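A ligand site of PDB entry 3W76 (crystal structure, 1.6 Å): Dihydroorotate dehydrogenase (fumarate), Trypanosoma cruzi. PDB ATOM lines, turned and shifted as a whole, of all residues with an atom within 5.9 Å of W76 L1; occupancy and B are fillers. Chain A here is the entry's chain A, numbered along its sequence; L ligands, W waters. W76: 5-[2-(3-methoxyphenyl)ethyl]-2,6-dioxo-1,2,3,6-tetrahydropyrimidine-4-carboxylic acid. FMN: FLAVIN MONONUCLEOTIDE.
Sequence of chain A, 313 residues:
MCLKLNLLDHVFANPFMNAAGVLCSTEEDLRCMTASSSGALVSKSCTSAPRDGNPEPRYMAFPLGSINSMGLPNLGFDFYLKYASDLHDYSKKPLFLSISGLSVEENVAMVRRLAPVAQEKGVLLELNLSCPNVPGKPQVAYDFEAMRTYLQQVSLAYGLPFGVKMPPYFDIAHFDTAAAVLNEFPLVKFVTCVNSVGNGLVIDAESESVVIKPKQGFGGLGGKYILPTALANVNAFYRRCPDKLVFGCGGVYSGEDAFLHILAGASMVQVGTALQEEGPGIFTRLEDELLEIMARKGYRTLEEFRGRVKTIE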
ATOM      1  N   LYS A  44      19.957  22.507  -9.477  1.00  0.00           N
ATOM      2  CA  LYS A  44      19.452  21.808  -8.308  1.00  0.00           C
ATOM      3  C   LYS A  44      20.626  21.453  -7.438  1.00  0.00           C
ATOM      4  O   LYS A  44      21.658  21.002  -7.909  1.00  0.00           O
ATOM      5  CB  LYS A  44      18.768  20.501  -8.774  1.00  0.00           C
ATOM      6  CG  LYS A  44      18.363  19.559  -7.639  1.00  0.00           C
ATOM      7  CD  LYS A  44      17.276  20.059  -6.685  1.00  0.00           C
ATOM      8  CE  LYS A  44      17.110  19.213  -5.424  1.00  0.00           C
ATOM      9  NZ  LYS A  44      16.083  19.790  -4.517  1.00  0.00           N
ATOM     10  N   SER A  45      20.475  21.545  -6.111  1.00  0.00           N
ATOM     11  CA  SER A  45      21.571  21.195  -5.234  1.00  0.00           C
ATOM     12  C   SER A  45      21.865  19.710  -5.456  1.00  0.00           C
ATOM     13  O   SER A  45      20.980  18.868  -5.485  1.00  0.00           O
ATOM     14  CB  SER A  45      21.208  21.337  -3.768  1.00  0.00           C
ATOM     15  OG  SER A  45      21.061  22.704  -3.416  1.00  0.00           O
ATOM     16  N   ASN A  54      12.549  11.712  -1.892  1.00  0.00           N
ATOM     17  CA  ASN A  54      11.509  11.151  -1.086  1.00  0.00           C
ATOM     18  C   ASN A  54      10.298  10.731  -1.867  1.00  0.00           C
ATOM     19  O   ASN A  54      10.080  11.108  -3.009  1.00  0.00           O
ATOM     20  CB  ASN A  54      11.096  12.235  -0.037  1.00  0.00           C
ATOM     21  CG  ASN A  54      12.079  12.392   1.055  1.00  0.00           C
ATOM     22  OD1 ASN A  54      12.909  11.479   1.314  1.00  0.00           O
ATOM     23  ND2 ASN A  54      12.037  13.502   1.770  1.00  0.00           N
ATOM     24  N   ASN A  68       7.521  21.715   1.009  1.00  0.00           N
ATOM     25  CA  ASN A  68       8.247  20.628   0.297  1.00  0.00           C
ATOM     26  C   ASN A  68       9.082  19.838   1.273  1.00  0.00           C
ATOM     27  O   ASN A  68       9.769  20.370   2.145  1.00  0.00           O
ATOM     28  CB  ASN A  68       9.069  21.164  -0.852  1.00  0.00           C
ATOM     29  CG  ASN A  68      10.470  21.599  -0.498  1.00  0.00           C
ATOM     30  OD1 ASN A  68      11.403  20.811  -0.365  1.00  0.00           O
ATOM     31  ND2 ASN A  68      10.622  22.849  -0.262  1.00  0.00           N
ATOM     32  N   SER A  69       9.149  18.510   0.947  1.00  0.00           N
ATOM     33  CA  SER A  69      10.180  17.635   1.527  1.00  0.00           C
ATOM     34  C   SER A  69      10.730  16.796   0.385  1.00  0.00           C
ATOM     35  O   SER A  69      10.463  15.598   0.330  1.00  0.00           O
ATOM     36  CB  SER A  69       9.542  16.767   2.560  1.00  0.00           C
ATOM     37  OG  SER A  69      10.551  15.938   3.179  1.00  0.00           O
ATOM     38  N   MET A  70      11.406  17.431  -0.567  1.00  0.00           N
ATOM     39  CA  MET A  70      11.807  16.754  -1.756  1.00  0.00           C
ATOM     40  C   MET A  70      12.783  15.634  -1.452  1.00  0.00           C
ATOM     41  O   MET A  70      12.693  14.586  -2.142  1.00  0.00           O
ATOM     42  CB  MET A  70      12.368  17.698  -2.765  1.00  0.00           C
ATOM     43  CG  MET A  70      11.569  18.883  -3.226  1.00  0.00           C
ATOM     44  SD  MET A  70       9.978  18.461  -3.889  1.00  0.00           S
ATOM     45  CE  MET A  70      10.428  17.864  -5.427  1.00  0.00           C
ATOM     46  N   GLY A  71      13.672  15.833  -0.534  1.00  0.00           N
ATOM     47  CA  GLY A  71      14.744  14.895  -0.238  1.00  0.00           C
ATOM     48  C   GLY A  71      15.924  14.892  -1.123  1.00  0.00           C
ATOM     49  O   GLY A  71      16.606  13.854  -1.311  1.00  0.00           O
ATOM     50  N   LEU A  72      16.308  16.058  -1.635  1.00  0.00           N
ATOM     51  CA  LEU A  72      17.430  16.223  -2.512  1.00  0.00           C
ATOM     52  C   LEU A  72      17.436  15.278  -3.704  1.00  0.00           C
ATOM     53  O   LEU A  72      18.509  14.737  -4.060  1.00  0.00           O
ATOM     54  CB  LEU A  72      18.681  16.159  -1.658  1.00  0.00           C
ATOM     55  CG  LEU A  72      19.991  16.778  -1.877  1.00  0.00           C
ATOM     56  CD1 LEU A  72      19.899  18.212  -2.379  1.00  0.00           C
ATOM     57  CD2 LEU A  72      20.659  16.679  -0.470  1.00  0.00           C
ATOM     58  N   PRO A  73      16.339  15.142  -4.427  1.00  0.00           N
ATOM     59  CA  PRO A  73      16.386  14.356  -5.689  1.00  0.00           C
ATOM     60  C   PRO A  73      17.295  15.099  -6.632  1.00  0.00           C
ATOM     61  O   PRO A  73      17.127  16.335  -6.807  1.00  0.00           O
ATOM     62  CB  PRO A  73      14.936  14.336  -6.197  1.00  0.00           C
ATOM     63  CG  PRO A  73      14.359  15.486  -5.505  1.00  0.00           C
ATOM     64  CD  PRO A  73      15.069  15.868  -4.278  1.00  0.00           C
ATOM     65  N   SER A 100      25.184  20.359  -2.281  1.00  0.00           N
ATOM     66  CA  SER A 100      24.698  20.034  -0.995  1.00  0.00           C
ATOM     67  C   SER A 100      25.129  18.616  -0.654  1.00  0.00           C
ATOM     68  O   SER A 100      24.326  17.751  -0.461  1.00  0.00           O
ATOM     69  CB  SER A 100      23.144  20.186  -0.897  1.00  0.00           C
ATOM     70  OG  SER A 100      22.816  20.047   0.438  1.00  0.00           O
ATOM     71  N   ASN A 128      25.105  24.981  -0.470  1.00  0.00           N
ATOM     72  CA  ASN A 128      23.907  24.865   0.340  1.00  0.00           C
ATOM     73  C   ASN A 128      24.183  24.263   1.689  1.00  0.00           C
ATOM     74  O   ASN A 128      24.523  23.096   1.737  1.00  0.00           O
ATOM     75  CB  ASN A 128      22.872  24.040  -0.433  1.00  0.00           C
ATOM     76  CG  ASN A 128      21.557  23.872   0.300  1.00  0.00           C
ATOM     77  OD1 ASN A 128      21.324  24.389   1.376  1.00  0.00           O
ATOM     78  ND2 ASN A 128      20.705  23.088  -0.255  1.00  0.00           N
ATOM     79  N   SER A 130      22.003  23.599   4.031  1.00  0.00           N
ATOM     80  CA  SER A 130      20.850  22.793   4.554  1.00  0.00           C
ATOM     81  C   SER A 130      20.835  21.357   4.013  1.00  0.00           C
ATOM     82  O   SER A 130      21.154  21.084   2.826  1.00  0.00           O
ATOM     83  CB  SER A 130      19.531  23.524   4.160  1.00  0.00           C
ATOM     84  OG  SER A 130      19.446  24.826   4.705  1.00  0.00           O
ATOM     85  N   CYS A 131      20.413  20.379   4.815  1.00  0.00           N
ATOM     86  CA  CYS A 131      20.468  18.971   4.428  1.00  0.00           C
ATOM     87  C   CYS A 131      19.376  18.196   5.158  1.00  0.00           C
ATOM     88  O   CYS A 131      18.865  18.651   6.185  1.00  0.00           O
ATOM     89  CB  CYS A 131      21.851  18.329   4.774  1.00  0.00           C
ATOM     90  SG  CYS A 131      22.370  18.347   6.504  1.00  0.00           S
ATOM     91  N   PRO A 132      19.037  17.025   4.642  1.00  0.00           N
ATOM     92  CA  PRO A 132      18.086  16.187   5.428  1.00  0.00           C
ATOM     93  C   PRO A 132      18.517  15.996   6.877  1.00  0.00           C
ATOM     94  O   PRO A 132      19.711  15.826   7.141  1.00  0.00           O
ATOM     95  CB  PRO A 132      18.088  14.872   4.625  1.00  0.00           C
ATOM     96  CG  PRO A 132      18.373  15.242   3.232  1.00  0.00           C
ATOM     97  CD  PRO A 132      19.439  16.339   3.390  1.00  0.00           C
ATOM     98  N   ASN A 133      17.516  15.945   7.785  1.00  0.00           N
ATOM     99  CA  ASN A 133      17.694  15.850   9.215  1.00  0.00           C
ATOM    100  C   ASN A 133      18.472  14.516   9.475  1.00  0.00           C
ATOM    101  O   ASN A 133      18.143  13.447   8.943  1.00  0.00           O
ATOM    102  CB  ASN A 133      16.328  15.776   9.961  1.00  0.00           C
ATOM    103  CG  ASN A 133      16.435  15.396  11.475  1.00  0.00           C
ATOM    104  OD1 ASN A 133      15.783  14.445  11.941  1.00  0.00           O
ATOM    105  ND2 ASN A 133      17.167  16.212  12.283  1.00  0.00           N
ATOM    106  N   GLN A 139      20.811  21.203  11.836  1.00  0.00           N
ATOM    107  CA  GLN A 139      21.299  21.670  10.567  1.00  0.00           C
ATOM    108  C   GLN A 139      22.646  22.420  10.758  1.00  0.00           C
ATOM    109  O   GLN A 139      22.798  23.161  11.697  1.00  0.00           O
ATOM    110  CB  GLN A 139      20.237  22.679  10.013  1.00  0.00           C
ATOM    111  CG  GLN A 139      18.945  21.931   9.723  1.00  0.00           C
ATOM    112  CD  GLN A 139      19.107  21.046   8.517  1.00  0.00           C
ATOM    113  OE1 GLN A 139      19.440  21.553   7.446  1.00  0.00           O
ATOM    114  NE2 GLN A 139      18.947  19.712   8.680  1.00  0.00           N
ATOM    115  N   LYS A 165      24.252  29.420   0.521  1.00  0.00           N
ATOM    116  CA  LYS A 165      22.758  29.436   0.736  1.00  0.00           C
ATOM    117  C   LYS A 165      22.483  29.154   2.237  1.00  0.00           C
ATOM    118  O   LYS A 165      22.839  28.095   2.751  1.00  0.00           O
ATOM    119  CB  LYS A 165      22.105  28.430  -0.178  1.00  0.00           C
ATOM    120  CG  LYS A 165      20.573  28.320  -0.048  1.00  0.00           C
ATOM    121  CD  LYS A 165      19.957  29.467  -0.708  1.00  0.00           C
ATOM    122  CE  LYS A 165      18.463  29.292  -0.820  1.00  0.00           C
ATOM    123  NZ  LYS A 165      18.064  28.336  -1.862  1.00  0.00           N
ATOM    124  N   ASN A 195      16.910  30.023   2.347  1.00  0.00           N
ATOM    125  CA  ASN A 195      16.244  28.760   2.102  1.00  0.00           C
ATOM    126  C   ASN A 195      14.844  28.746   2.707  1.00  0.00           C
ATOM    127  O   ASN A 195      14.402  29.697   3.410  1.00  0.00           O
ATOM    128  CB  ASN A 195      17.126  27.619   2.650  1.00  0.00           C
ATOM    129  CG  ASN A 195      17.052  26.379   1.795  1.00  0.00           C
ATOM    130  OD1 ASN A 195      15.975  25.907   1.425  1.00  0.00           O
ATOM    131  ND2 ASN A 195      18.232  25.777   1.510  1.00  0.00           N
ATOM    132  N   SER A 196      14.079  27.690   2.459  1.00  0.00           N
ATOM    133  CA  SER A 196      12.724  27.532   2.956  1.00  0.00           C
ATOM    134  C   SER A 196      12.720  27.587   4.494  1.00  0.00           C
ATOM    135  O   SER A 196      13.726  27.289   5.177  1.00  0.00           O
ATOM    136  CB  SER A 196      12.088  26.240   2.350  1.00  0.00           C
ATOM    137  OG  SER A 196      12.823  25.146   2.692  1.00  0.00           O
ATOM    138  N   LYS A 215       8.151  12.625   6.213  1.00  0.00           N
ATOM    139  CA  LYS A 215       8.309  13.418   7.456  1.00  0.00           C
ATOM    140  C   LYS A 215       6.993  13.695   8.184  1.00  0.00           C
ATOM    141  O   LYS A 215       6.854  14.699   8.836  1.00  0.00           O
ATOM    142  CB  LYS A 215       9.095  14.750   7.200  1.00  0.00           C
ATOM    143  CG  LYS A 215      10.474  14.618   6.662  1.00  0.00           C
ATOM    144  CD  LYS A 215      11.217  15.980   6.431  1.00  0.00           C
ATOM    145  CE  LYS A 215      11.172  16.897   7.629  1.00  0.00           C
ATOM    146  NZ  LYS A 215      12.008  18.064   7.418  1.00  0.00           N
ATOM    147  N   GLY A 220       9.706  22.201   4.311  1.00  0.00           N
ATOM    148  CA  GLY A 220      10.070  23.615   4.263  1.00  0.00           C
ATOM    149  C   GLY A 220       9.021  24.431   3.585  1.00  0.00           C
ATOM    150  O   GLY A 220       8.450  24.085   2.563  1.00  0.00           O
HETATM  151  OAJ W76 L   1      14.007  18.877  -0.078  1.00  0.00           O
HETATM  152  CAI W76 L   1      14.915  19.405  -0.816  1.00  0.00           C
HETATM  153  OAK W76 L   1      15.492  18.833  -1.798  1.00  0.00           O
HETATM  154  C4  W76 L   1      15.305  20.760  -0.391  1.00  0.00           C
HETATM  155  N3  W76 L   1      14.183  21.594  -0.161  1.00  0.00           N
HETATM  156  C2  W76 L   1      14.364  22.869   0.309  1.00  0.00           C
HETATM  157  O2  W76 L   1      13.359  23.638   0.499  1.00  0.00           O
HETATM  158  N1  W76 L   1      15.620  23.335   0.464  1.00  0.00           N
HETATM  159  C6  W76 L   1      16.743  22.554   0.224  1.00  0.00           C
HETATM  160  O6  W76 L   1      17.824  23.070   0.460  1.00  0.00           O
HETATM  161  C5  W76 L   1      16.576  21.238  -0.215  1.00  0.00           C
HETATM  162  CAL W76 L   1      17.728  20.321  -0.440  1.00  0.00           C
HETATM  163  CAM W76 L   1      18.429  20.077   0.860  1.00  0.00           C
HETATM  164  CAN W76 L   1      17.551  19.531   1.806  1.00  0.00           C
HETATM  165  CAS W76 L   1      16.706  18.419   1.629  1.00  0.00           C
HETATM  166  CAO W76 L   1      17.347  20.142   3.041  1.00  0.00           C
HETATM  167  CAP W76 L   1      16.446  19.702   4.003  1.00  0.00           C
HETATM  168  CAQ W76 L   1      15.662  18.583   3.861  1.00  0.00           C
HETATM  169  CAR W76 L   1      15.795  17.947   2.607  1.00  0.00           C
HETATM  170  OAT W76 L   1      15.100  16.877   2.190  1.00  0.00           O
HETATM  171  CAU W76 L   1      13.851  16.528   2.840  1.00  0.00           C
HETATM  172  N1  FMN L   2      17.004  25.300  -1.924  1.00  0.00           N
HETATM  173  C2  FMN L   2      18.263  24.888  -2.152  1.00  0.00           C
HETATM  174  O2  FMN L   2      19.203  25.660  -1.866  1.00  0.00           O
HETATM  175  N3  FMN L   2      18.539  23.756  -2.835  1.00  0.00           N
HETATM  176  C4  FMN L   2      17.614  22.947  -3.293  1.00  0.00           C
HETATM  177  O4  FMN L   2      17.836  21.915  -3.991  1.00  0.00           O
HETATM  178  C4A FMN L   2      16.232  23.339  -3.099  1.00  0.00           C
HETATM  179  N5  FMN L   2      15.215  22.586  -3.559  1.00  0.00           N
HETATM  180  C5A FMN L   2      13.985  23.127  -3.549  1.00  0.00           C
HETATM  181  C6  FMN L   2      12.921  22.417  -4.085  1.00  0.00           C
HETATM  182  C7  FMN L   2      11.605  22.941  -4.089  1.00  0.00           C
HETATM  183  C7M FMN L   2      10.452  22.180  -4.780  1.00  0.00           C
HETATM  184  C8  FMN L   2      11.327  24.158  -3.414  1.00  0.00           C
HETATM  185  C8M FMN L   2       9.982  24.733  -3.309  1.00  0.00           C
HETATM  186  C9  FMN L   2      12.395  24.821  -2.816  1.00  0.00           C
HETATM  187  C9A FMN L   2      13.667  24.343  -2.853  1.00  0.00           C
HETATM  188  N10 FMN L   2      14.698  25.031  -2.242  1.00  0.00           N
HETATM  189  C10 FMN L   2      16.013  24.608  -2.428  1.00  0.00           C
HETATM  190  C1' FMN L   2      14.534  26.288  -1.529  1.00  0.00           C
HETATM  191  C2' FMN L   2      14.378  27.420  -2.528  1.00  0.00           C
HETATM  192  O2' FMN L   2      15.586  27.625  -3.231  1.00  0.00           O
HETATM  193  C3' FMN L   2      14.015  28.734  -1.824  1.00  0.00           C
HETATM  194  O3' FMN L   2      15.108  29.028  -0.917  1.00  0.00           O
HETATM  195  C4' FMN L   2      12.695  28.695  -1.016  1.00  0.00           C
HETATM  196  O4' FMN L   2      11.678  27.954  -1.751  1.00  0.00           O
HETATM  197  C5' FMN L   2      12.199  30.089  -0.691  1.00  0.00           C
HETATM  198  O5' FMN L   2      11.926  30.889  -1.824  1.00  0.00           O
HETATM  199  P   FMN L   2      10.399  31.075  -2.331  1.00  0.00           P
HETATM  200  O1P FMN L   2      10.559  31.855  -3.580  1.00  0.00           O
HETATM  201  O2P FMN L   2       9.653  31.754  -1.227  1.00  0.00           O
HETATM  202  O3P FMN L   2       9.852  29.687  -2.652  1.00  0.00           O
HETATM  203  O   HOH W   1      13.617  13.324   4.193  1.00  0.00           O
HETATM  204  O   HOH W   2      12.731  19.956   2.222  1.00  0.00           O
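ND2 of Asn 195 is in hydrogen-bond range of OD1 of Asn 128, at 3.4 Å. OD1 of Asn 68 is in hydrogen-bond range of N of Met 70 (3.4 Å). N of Gly 220 is in hydrogen-bond range of O of Asn 68, at 2.8 Å. OD1 of Asn 128 lies within hydrogen-bond range of N of Ser 130 (2.9 Å). The side-chain hydroxyl (OG) of Ser 45 is in hydrogen-bond range of the side-chain amide nitrogen (ND2) of Asn 128. The backbone carbonyl oxygen (O) of Met 70 is in hydrogen-bond range of the backbone NH (N) of Asn 54 (2.9 Å). The side-chain amide nitrogen of Asn 54 is in hydrogen-bond range of the backbone carbonyl oxygen of Ser 69 (3.0 Å). The backbone carbonyl oxygen of Ser 130 is in hydrogen-bond range of the side-chain hydroxyl of Ser 100.
The side-chain hydroxyl (OG) of Ser 196 sits at hydrogen-bond distance from an oxygen (O2) of W76 L1 (2.7 Å). N1 of W76 L1 sits at hydrogen-bond distance from OD1 of Asn 195 (2.8 Å). The side-chain amide oxygen (OD1) of Asn 68 sits at hydrogen-bond distance from a nitrogen (N3) of W76 L1. The backbone NH (N) of Leu 72 lies within hydrogen-bond range of an oxygen (OAK) of W76 L1 (2.9 Å). NZ of Lys 44 is in salt-bridge range of OAK of W76 L1. ND2 of Asn 128 lies within hydrogen-bond range of O6 of W76 L1 (3.0 Å). The backbone NH (N) of Met 70 is in hydrogen-bond range of an oxygen (OAJ) of W76 L1. An oxygen (OAJ) of W76 L1 is in hydrogen-bond range of the backbone NH (N) of Gly 71, at 3.1 Å. The side-chain amino group of Lys 44 lies within hydrogen-bond range of an oxygen (O4) of FMN L2, at 2.8 Å. The side-chain amide nitrogen (ND2) of Asn 128 sits at hydrogen-bond distance from an oxygen (O2) of FMN L2, 3.4 Å away. N of Ser 45 is in hydrogen-bond range of O4 of FMN L2 (3.4 Å). The side-chain hydroxyl of Ser 45 lies within hydrogen-bond range of a nitrogen (N3) of FMN L2, at 2.8 Å. An oxygen (O2) of FMN L2 is in hydrogen-bond range of the side-chain amino group (NZ) of Lys 165, 2.9 Å away.
A nitrogen (N1) of W76 L1 lies close to a nitrogen (N1) of FMN L2, at 3.4 Å.
ND2 of Asn 54 touches CAU of W76 L1 (3.7 Å). Ser 69 touches W76 L1 (OG to CAU, 3.4 Å). CD of Pro 73 touches OAK of W76 L1, 3.9 Å away. Ser 130 touches W76 L1. O of Cys 131 touches CAP of W76 L1 (3.4 Å). Pro 132 touches W76 L1. The nearest printed residue that does not touch W76 L1 is Ser 100 (4.4 Å).
Water W2 lies within hydrogen-bond range of OAJ of W76 L1 and O of Asn 68.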
